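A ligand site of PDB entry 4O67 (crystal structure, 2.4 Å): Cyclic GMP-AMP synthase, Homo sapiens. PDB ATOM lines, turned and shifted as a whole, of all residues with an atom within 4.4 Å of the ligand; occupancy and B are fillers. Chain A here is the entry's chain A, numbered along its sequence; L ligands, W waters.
Water W2 lies within hydrogen-bond range of the side-chain hydroxyl (OG) of Ser 219 (2.4 Å) and an oxygen (O11) of the ligand (2.9 Å).
Water W1 bridges a ring nitrogen (NE2) of His 278 and the backbone carbonyl oxygen (O) of Leu 331.
An oxygen (O10) of the ligand sits close to the backbone NH (N) of Ser 146, at 3.5 Å.
OD2 of Asp 160 lies within hydrogen-bond range of N9 of the ligand.
The side-chain carboxylate (OD1) of Asp 68 is in hydrogen-bond range of a nitrogen (N9) of the ligand (3.0 Å).
The guanidinium group of Arg 217 lies within hydrogen-bond range of an oxygen (O11) of the ligand.
An oxygen (O3) of the ligand lies within hydrogen-bond range of the side-chain hydroxyl (OG) of Ser 275, 2.9 Å away.
The side-chain hydroxyl (OH) of Tyr 277 lies close to a nitrogen (N2) of the ligand.
OG of Ser 146 sits close to O10 of the ligand (3.3 Å).
An oxygen (O9) of the ligand lies within salt-bridge range of the side-chain amino group of Lys 203, at 2.8 Å.
CD of Lys 142 touches O5 of the ligand (3.6 Å).
Arg 143 touches the ligand (CD to O5, 3.6 Å).
O of Gly 144 touches C14 of the ligand, 3.8 Å away.
Pro 147 touches the ligand (CD to N7, 3.7 Å).
CB of Ala 148 touches N9 of the ligand, at 3.9 Å.
Thr 162 touches the ligand (OG1 to N9, 3.9 Å).
OG of Ser 219 touches N1 of the ligand, at 3.9 Å.
His 278 touches the ligand (NE2 to C10, 3.8 Å).
Asn 323 touches the ligand (ND2 to C1, 3.98 Å).
Leu 336 touches the ligand (CD2 to O9, 3.9 Å).
Hydrophobic or aromatic side chains that line the ligand: Pro 147, Ala 148, Tyr 277, His 278 and Leu 336.
Within 4 Å of the ligand: Asp 68, Lys 142, Arg 143, Gly 144, Ser 146, Pro 147, Ala 148, Asp 160, Thr 162, Lys 203, Arg 217, Ser 219, Ser 275, Tyr 277, His 278, Asn 323 and Leu 336.
The nearest printed residue that does not touch the ligand is Leu 331 (4.2 Å).
The backbone carbonyl oxygen (O) of Leu 336 is in hydrogen-bond range of the side-chain amino group (NZ) of Lys 273, 3.4 Å away.
OG of Ser 146 lies close to N of Ala 148 (3.1 Å).
OD1 of Asp 160 lies within salt-bridge range of NZ of Lys 142 (3.3 Å).
The side-chain hydroxyl of Ser 275 lies close to the backbone NH of Tyr 277, 3.3 Å away.
ND1 of His 278 sits at hydrogen-bond distance from N of Ser 275.
The backbone carbonyl oxygen of Phe 329 is in hydrogen-bond range of the backbone NH of Asn 323, at 2.9 Å.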
ATOM      1  N   ASP A  68     -28.950  23.300  20.775  1.00  0.00           N
ATOM      2  CA  ASP A  68     -27.542  23.265  20.438  1.00  0.00           C
ATOM      3  C   ASP A  68     -27.270  23.410  18.942  1.00  0.00           C
ATOM      4  O   ASP A  68     -27.676  22.557  18.139  1.00  0.00           O
ATOM      5  CB  ASP A  68     -26.921  21.979  20.968  1.00  0.00           C
ATOM      6  CG  ASP A  68     -25.496  21.814  20.524  1.00  0.00           C
ATOM      7  OD1 ASP A  68     -24.615  22.479  21.101  1.00  0.00           O
ATOM      8  OD2 ASP A  68     -25.256  21.017  19.583  1.00  0.00           O
ATOM      9  N   TYR A  89      -7.360  17.295  22.693  1.00  0.00           N
ATOM     10  CA  TYR A  89      -7.019  18.720  22.480  1.00  0.00           C
ATOM     11  C   TYR A  89      -5.757  18.936  21.654  1.00  0.00           C
ATOM     12  O   TYR A  89      -4.838  18.141  21.684  1.00  0.00           O
ATOM     13  CB  TYR A  89      -6.876  19.436  23.802  1.00  0.00           C
ATOM     14  CG  TYR A  89      -8.122  19.368  24.649  1.00  0.00           C
ATOM     15  CD1 TYR A  89      -8.354  18.288  25.499  1.00  0.00           C
ATOM     16  CD2 TYR A  89      -9.082  20.379  24.597  1.00  0.00           C
ATOM     17  CE1 TYR A  89      -9.513  18.233  26.286  1.00  0.00           C
ATOM     18  CE2 TYR A  89     -10.226  20.335  25.372  1.00  0.00           C
ATOM     19  CZ  TYR A  89     -10.435  19.260  26.206  1.00  0.00           C
ATOM     20  OH  TYR A  89     -11.577  19.209  26.969  1.00  0.00           O
ATOM     21  N   LYS A 142     -22.313  29.636  30.433  1.00  0.00           N
ATOM     22  CA  LYS A 142     -22.768  28.378  31.018  1.00  0.00           C
ATOM     23  C   LYS A 142     -21.813  27.916  32.100  1.00  0.00           C
ATOM     24  O   LYS A 142     -22.181  27.723  33.254  1.00  0.00           O
ATOM     25  CB  LYS A 142     -22.897  27.304  29.933  1.00  0.00           C
ATOM     26  CG  LYS A 142     -23.250  25.910  30.466  1.00  0.00           C
ATOM     27  CD  LYS A 142     -23.157  24.847  29.388  1.00  0.00           C
ATOM     28  CE  LYS A 142     -24.122  25.142  28.248  1.00  0.00           C
ATOM     29  NZ  LYS A 142     -25.557  25.053  28.655  1.00  0.00           N
ATOM     30  N   ARG A 143     -20.590  27.670  31.680  1.00  0.00           N
ATOM     31  CA  ARG A 143     -19.569  27.191  32.562  1.00  0.00           C
ATOM     32  C   ARG A 143     -18.262  27.514  31.863  1.00  0.00           C
ATOM     33  O   ARG A 143     -18.225  27.659  30.634  1.00  0.00           O
ATOM     34  CB  ARG A 143     -19.735  25.686  32.824  1.00  0.00           C
ATOM     35  CG  ARG A 143     -18.688  25.032  33.697  1.00  0.00           C
ATOM     36  CD  ARG A 143     -19.018  23.560  33.848  1.00  0.00           C
ATOM     37  NE  ARG A 143     -20.235  23.334  34.621  1.00  0.00           N
ATOM     38  CZ  ARG A 143     -20.276  23.092  35.924  1.00  0.00           C
ATOM     39  NH1 ARG A 143     -19.143  23.012  36.611  1.00  0.00           N
ATOM     40  NH2 ARG A 143     -21.432  22.898  36.543  1.00  0.00           N
ATOM     41  N   GLY A 144     -17.213  27.710  32.636  1.00  0.00           N
ATOM     42  CA  GLY A 144     -15.883  27.860  32.087  1.00  0.00           C
ATOM     43  C   GLY A 144     -15.562  26.621  31.275  1.00  0.00           C
ATOM     44  O   GLY A 144     -16.075  25.547  31.563  1.00  0.00           O
ATOM     45  N   GLY A 145     -14.777  26.791  30.219  1.00  0.00           N
ATOM     46  CA  GLY A 145     -14.302  25.687  29.397  1.00  0.00           C
ATOM     47  C   GLY A 145     -15.073  25.559  28.102  1.00  0.00           C
ATOM     48  O   GLY A 145     -14.483  25.260  27.074  1.00  0.00           O
ATOM     49  N   SER A 146     -16.382  25.818  28.166  1.00  0.00           N
ATOM     50  CA  SER A 146     -17.266  25.625  27.027  1.00  0.00           C
ATOM     51  C   SER A 146     -16.843  26.395  25.794  1.00  0.00           C
ATOM     52  O   SER A 146     -16.539  27.587  25.875  1.00  0.00           O
ATOM     53  CB  SER A 146     -18.689  26.010  27.396  1.00  0.00           C
ATOM     54  OG  SER A 146     -19.564  25.686  26.327  1.00  0.00           O
ATOM     55  N   PRO A 147     -16.818  25.710  24.645  1.00  0.00           N
ATOM     56  CA  PRO A 147     -16.548  26.291  23.330  1.00  0.00           C
ATOM     57  C   PRO A 147     -17.806  26.940  22.794  1.00  0.00           C
ATOM     58  O   PRO A 147     -17.852  27.433  21.678  1.00  0.00           O
ATOM     59  CB  PRO A 147     -16.184  25.077  22.488  1.00  0.00           C
ATOM     60  CG  PRO A 147     -17.037  23.994  23.066  1.00  0.00           C
ATOM     61  CD  PRO A 147     -17.090  24.258  24.560  1.00  0.00           C
ATOM     62  N   ALA A 148     -18.843  26.918  23.628  1.00  0.00           N
ATOM     63  CA  ALA A 148     -20.138  27.424  23.242  1.00  0.00           C
ATOM     64  C   ALA A 148     -20.362  28.806  23.839  1.00  0.00           C
ATOM     65  O   ALA A 148     -19.935  29.090  24.959  1.00  0.00           O
ATOM     66  CB  ALA A 148     -21.235  26.445  23.695  1.00  0.00           C
ATOM     67  N   ASP A 160     -27.078  26.993  22.817  1.00  0.00           N
ATOM     68  CA  ASP A 160     -25.632  26.864  22.767  1.00  0.00           C
ATOM     69  C   ASP A 160     -25.225  27.037  21.323  1.00  0.00           C
ATOM     70  O   ASP A 160     -25.590  26.216  20.476  1.00  0.00           O
ATOM     71  CB  ASP A 160     -25.139  25.515  23.306  1.00  0.00           C
ATOM     72  CG  ASP A 160     -24.829  25.546  24.801  1.00  0.00           C
ATOM     73  OD1 ASP A 160     -25.537  26.254  25.559  1.00  0.00           O
ATOM     74  OD2 ASP A 160     -23.858  24.867  25.219  1.00  0.00           O
ATOM     75  N   THR A 162     -22.031  27.090  18.985  1.00  0.00           N
ATOM     76  CA  THR A 162     -20.640  26.686  19.015  1.00  0.00           C
ATOM     77  C   THR A 162     -19.924  26.951  17.691  1.00  0.00           C
ATOM     78  O   THR A 162     -20.371  26.531  16.624  1.00  0.00           O
ATOM     79  CB  THR A 162     -20.525  25.189  19.341  1.00  0.00           C
ATOM     80  OG1 THR A 162     -21.228  24.902  20.551  1.00  0.00           O
ATOM     81  CG2 THR A 162     -19.064  24.784  19.446  1.00  0.00           C
ATOM     82  N   LYS A 203     -12.725  24.737  22.681  1.00  0.00           N
ATOM     83  CA  LYS A 203     -12.741  24.289  24.064  1.00  0.00           C
ATOM     84  C   LYS A 203     -11.295  24.037  24.512  1.00  0.00           C
ATOM     85  O   LYS A 203     -10.618  23.187  23.913  1.00  0.00           O
ATOM     86  CB  LYS A 203     -13.599  23.022  24.183  1.00  0.00           C
ATOM     87  CG  LYS A 203     -13.213  22.018  25.250  1.00  0.00           C
ATOM     88  CD  LYS A 203     -13.644  22.487  26.612  1.00  0.00           C
ATOM     89  CE  LYS A 203     -12.971  21.709  27.727  1.00  0.00           C
ATOM     90  NZ  LYS A 203     -13.431  22.151  29.051  1.00  0.00           N
ATOM     91  N   ARG A 217     -10.528  21.266  20.672  1.00  0.00           N
ATOM     92  CA  ARG A 217     -10.746  19.829  20.707  1.00  0.00           C
ATOM     93  C   ARG A 217     -11.667  19.308  19.631  1.00  0.00           C
ATOM     94  O   ARG A 217     -12.483  20.046  19.041  1.00  0.00           O
ATOM     95  CB  ARG A 217     -11.241  19.358  22.063  1.00  0.00           C
ATOM     96  CG  ARG A 217     -12.669  19.608  22.317  1.00  0.00           C
ATOM     97  CD  ARG A 217     -13.349  18.401  22.975  1.00  0.00           C
ATOM     98  NE  ARG A 217     -14.662  18.843  23.433  1.00  0.00           N
ATOM     99  CZ  ARG A 217     -15.712  19.038  22.640  1.00  0.00           C
ATOM    100  NH1 ARG A 217     -15.646  18.808  21.338  1.00  0.00           N
ATOM    101  NH2 ARG A 217     -16.837  19.476  23.164  1.00  0.00           N
ATOM    102  N   SER A 219     -14.472  17.403  17.598  1.00  0.00           N
ATOM    103  CA  SER A 219     -15.907  17.228  17.737  1.00  0.00           C
ATOM    104  C   SER A 219     -16.367  16.411  16.530  1.00  0.00           C
ATOM    105  O   SER A 219     -15.897  16.624  15.402  1.00  0.00           O
ATOM    106  CB  SER A 219     -16.644  18.564  17.824  1.00  0.00           C
ATOM    107  OG  SER A 219     -18.050  18.368  17.897  1.00  0.00           O
ATOM    108  N   SER A 221     -19.925  15.645  16.302  1.00  0.00           N
ATOM    109  CA  SER A 221     -21.365  15.626  16.511  1.00  0.00           C
ATOM    110  C   SER A 221     -22.168  15.426  15.185  1.00  0.00           C
ATOM    111  O   SER A 221     -23.309  14.935  15.199  1.00  0.00           O
ATOM    112  CB  SER A 221     -21.795  16.910  17.220  1.00  0.00           C
ATOM    113  OG  SER A 221     -21.372  18.028  16.479  1.00  0.00           O
ATOM    114  N   LYS A 273     -22.814  18.219  37.204  1.00  0.00           N
ATOM    115  CA  LYS A 273     -21.718  18.004  36.261  1.00  0.00           C
ATOM    116  C   LYS A 273     -22.049  16.966  35.163  1.00  0.00           C
ATOM    117  O   LYS A 273     -21.364  16.882  34.155  1.00  0.00           O
ATOM    118  CB  LYS A 273     -20.480  17.568  37.028  1.00  0.00           C
ATOM    119  CG  LYS A 273     -19.646  18.671  37.635  1.00  0.00           C
ATOM    120  CD  LYS A 273     -18.732  19.252  36.588  1.00  0.00           C
ATOM    121  CE  LYS A 273     -17.642  20.098  37.210  1.00  0.00           C
ATOM    122  NZ  LYS A 273     -16.653  20.500  36.171  1.00  0.00           N
ATOM    123  N   SER A 275     -24.345  15.330  32.139  1.00  0.00           N
ATOM    124  CA  SER A 275     -25.152  15.875  31.057  1.00  0.00           C
ATOM    125  C   SER A 275     -25.611  14.842  30.068  1.00  0.00           C
ATOM    126  O   SER A 275     -25.152  13.696  30.087  1.00  0.00           O
ATOM    127  CB  SER A 275     -24.371  16.919  30.289  1.00  0.00           C
ATOM    128  OG  SER A 275     -23.453  16.258  29.445  1.00  0.00           O
ATOM    129  N   TYR A 277     -24.857  14.432  27.078  1.00  0.00           N
ATOM    130  CA  TYR A 277     -23.729  13.857  26.336  1.00  0.00           C
ATOM    131  C   TYR A 277     -23.081  12.603  26.990  1.00  0.00           C
ATOM    132  O   TYR A 277     -22.607  11.712  26.289  1.00  0.00           O
ATOM    133  CB  TYR A 277     -22.633  14.903  26.107  1.00  0.00           C
ATOM    134  CG  TYR A 277     -21.645  14.458  25.070  1.00  0.00           C
ATOM    135  CD1 TYR A 277     -21.959  14.517  23.688  1.00  0.00           C
ATOM    136  CD2 TYR A 277     -20.412  13.909  25.454  1.00  0.00           C
ATOM    137  CE1 TYR A 277     -21.047  14.060  22.727  1.00  0.00           C
ATOM    138  CE2 TYR A 277     -19.504  13.444  24.497  1.00  0.00           C
ATOM    139  CZ  TYR A 277     -19.834  13.521  23.136  1.00  0.00           C
ATOM    140  OH  TYR A 277     -18.930  13.069  22.204  1.00  0.00           O
ATOM    141  N   HIS A 278     -23.033  12.546  28.321  1.00  0.00           N
ATOM    142  CA  HIS A 278     -22.510  11.351  28.991  1.00  0.00           C
ATOM    143  C   HIS A 278     -23.436  10.213  28.681  1.00  0.00           C
ATOM    144  O   HIS A 278     -22.997   9.100  28.381  1.00  0.00           O
ATOM    145  CB  HIS A 278     -22.431  11.548  30.514  1.00  0.00           C
ATOM    146  CG  HIS A 278     -21.516  12.645  30.933  1.00  0.00           C
ATOM    147  ND1 HIS A 278     -21.947  13.709  31.693  1.00  0.00           N
ATOM    148  CD2 HIS A 278     -20.199  12.855  30.688  1.00  0.00           C
ATOM    149  CE1 HIS A 278     -20.927  14.531  31.893  1.00  0.00           C
ATOM    150  NE2 HIS A 278     -19.855  14.040  31.300  1.00  0.00           N
ATOM    151  N   ASN A 323     -14.838   8.514  25.511  1.00  0.00           N
ATOM    152  CA  ASN A 323     -15.303   9.179  24.330  1.00  0.00           C
ATOM    153  C   ASN A 323     -15.444   8.138  23.226  1.00  0.00           C
ATOM    154  O   ASN A 323     -14.570   7.297  23.050  1.00  0.00           O
ATOM    155  CB  ASN A 323     -14.335  10.288  23.938  1.00  0.00           C
ATOM    156  CG  ASN A 323     -14.826  11.100  22.757  1.00  0.00           C
ATOM    157  OD1 ASN A 323     -14.899  10.596  21.630  1.00  0.00           O
ATOM    158  ND2 ASN A 323     -15.130  12.359  22.997  1.00  0.00           N
ATOM    159  N   PHE A 329      -9.731   9.094  25.918  1.00  0.00           N
ATOM    160  CA  PHE A 329     -10.269  10.283  26.590  1.00  0.00           C
ATOM    161  C   PHE A 329     -11.455   9.881  27.436  1.00  0.00           C
ATOM    162  O   PHE A 329     -12.530   9.622  26.893  1.00  0.00           O
ATOM    163  CB  PHE A 329     -10.681  11.345  25.594  1.00  0.00           C
ATOM    164  CG  PHE A 329     -11.032  12.655  26.236  1.00  0.00           C
ATOM    165  CD1 PHE A 329     -10.065  13.609  26.455  1.00  0.00           C
ATOM    166  CD2 PHE A 329     -12.316  12.909  26.659  1.00  0.00           C
ATOM    167  CE1 PHE A 329     -10.369  14.814  27.053  1.00  0.00           C
ATOM    168  CE2 PHE A 329     -12.632  14.111  27.265  1.00  0.00           C
ATOM    169  CZ  PHE A 329     -11.659  15.067  27.468  1.00  0.00           C
ATOM    170  N   LEU A 331     -14.427  10.548  29.819  1.00  0.00           N
ATOM    171  CA  LEU A 331     -15.344  11.626  30.227  1.00  0.00           C
ATOM    172  C   LEU A 331     -15.646  11.591  31.718  1.00  0.00           C
ATOM    173  O   LEU A 331     -16.171  12.562  32.273  1.00  0.00           O
ATOM    174  CB  LEU A 331     -16.667  11.552  29.443  1.00  0.00           C
ATOM    175  CG  LEU A 331     -16.619  11.556  27.920  1.00  0.00           C
ATOM    176  CD1 LEU A 331     -17.989  11.298  27.395  1.00  0.00           C
ATOM    177  CD2 LEU A 331     -16.078  12.853  27.382  1.00  0.00           C
ATOM    178  N   LEU A 336     -12.559  15.678  35.463  1.00  0.00           N
ATOM    179  CA  LEU A 336     -13.786  16.289  34.959  1.00  0.00           C
ATOM    180  C   LEU A 336     -14.910  16.242  35.987  1.00  0.00           C
ATOM    181  O   LEU A 336     -15.561  17.245  36.261  1.00  0.00           O
ATOM    182  CB  LEU A 336     -14.225  15.603  33.663  1.00  0.00           C
ATOM    183  CG  LEU A 336     -13.195  15.763  32.539  1.00  0.00           C
ATOM    184  CD1 LEU A 336     -13.551  14.992  31.282  1.00  0.00           C
ATOM    185  CD2 LEU A 336     -13.015  17.236  32.223  1.00  0.00           C
HETATM  186  C1  LIG L   1     -17.178  15.743  22.603  1.00  0.00           C
HETATM  187  N1  LIG L   1     -20.063  17.552  21.151  1.00  0.00           N
HETATM  188  C2  LIG L   1     -19.113  16.983  22.128  1.00  0.00           C
HETATM  189  N2  LIG L   1     -18.049  16.268  21.724  1.00  0.00           N
HETATM  190  N3  LIG L   1     -17.325  15.912  23.918  1.00  0.00           N
HETATM  191  C3  LIG L   1     -18.375  16.634  24.432  1.00  0.00           C
HETATM  192  C4  LIG L   1     -19.320  17.202  23.537  1.00  0.00           C
HETATM  193  N4  LIG L   1     -20.261  17.867  24.312  1.00  0.00           N
HETATM  194  C5  LIG L   1     -19.953  17.729  25.622  1.00  0.00           C
HETATM  195  N5  LIG L   1     -18.826  16.986  25.676  1.00  0.00           N
HETATM  196  C6  LIG L   1     -17.989  16.498  26.732  1.00  0.00           C
HETATM  197  C7  LIG L   1     -17.094  17.575  27.167  1.00  0.00           C
HETATM  198  O1  LIG L   1     -15.759  17.071  27.259  1.00  0.00           O
HETATM  199  C8  LIG L   1     -17.628  18.060  28.451  1.00  0.00           C
HETATM  200  C9  LIG L   1     -18.494  16.990  28.988  1.00  0.00           C
HETATM  201  C10 LIG L   1     -19.756  17.510  29.645  1.00  0.00           C
HETATM  202  O2  LIG L   1     -20.365  18.432  28.785  1.00  0.00           O
HETATM  203  P1  LIG L   1     -21.603  19.354  29.209  1.00  0.00           P
HETATM  204  O3  LIG L   1     -22.920  18.938  28.533  1.00  0.00           O
HETATM  205  O4  LIG L   1     -21.290  20.940  28.996  1.00  0.00           O
HETATM  206  C11 LIG L   1     -19.935  21.322  28.875  1.00  0.00           C
HETATM  207  C12 LIG L   1     -19.454  21.983  30.110  1.00  0.00           C
HETATM  208  O5  LIG L   1     -20.499  22.763  30.626  1.00  0.00           O
HETATM  209  C13 LIG L   1     -18.374  22.871  29.679  1.00  0.00           C
HETATM  210  C14 LIG L   1     -16.998  22.281  29.814  1.00  0.00           C
HETATM  211  O6  LIG L   1     -17.112  20.878  29.933  1.00  0.00           O
HETATM  212  P2  LIG L   1     -15.996  19.913  29.306  1.00  0.00           P
HETATM  213  O7  LIG L   1     -16.532  18.357  29.362  1.00  0.00           O
HETATM  214  O8  LIG L   1     -15.504  20.261  27.941  1.00  0.00           O
HETATM  215  O9  LIG L   1     -14.822  20.010  30.187  1.00  0.00           O
HETATM  216  O10 LIG L   1     -18.621  23.170  28.285  1.00  0.00           O
HETATM  217  C15 LIG L   1     -19.735  22.371  27.844  1.00  0.00           C
HETATM  218  N6  LIG L   1     -19.290  21.820  26.688  1.00  0.00           N
HETATM  219  C16 LIG L   1     -18.166  21.163  26.503  1.00  0.00           C
HETATM  220  N7  LIG L   1     -18.077  20.770  25.218  1.00  0.00           N
HETATM  221  C17 LIG L   1     -19.972  21.874  25.518  1.00  0.00           C
HETATM  222  C18 LIG L   1     -19.203  21.198  24.582  1.00  0.00           C
HETATM  223  C19 LIG L   1     -19.696  21.104  23.169  1.00  0.00           C
HETATM  224  N8  LIG L   1     -20.942  21.706  22.835  1.00  0.00           N
HETATM  225  C20 LIG L   1     -21.715  22.394  23.821  1.00  0.00           C
HETATM  226  N9  LIG L   1     -22.970  22.987  23.508  1.00  0.00           N
HETATM  227  N10 LIG L   1     -21.236  22.480  25.172  1.00  0.00           N
HETATM  228  O11 LIG L   1     -19.025  20.521  22.300  1.00  0.00           O
HETATM  229  O12 LIG L   1     -21.818  19.165  30.647  1.00  0.00           O
HETATM  230  O13 LIG L   1     -18.771  16.117  27.859  1.00  0.00           O
HETATM  231  O   HOH W   1     -17.222  14.936  31.156  1.00  0.00           O
HETATM  232  O   HOH W   2     -19.180  19.875  19.452  1.00  0.00           O
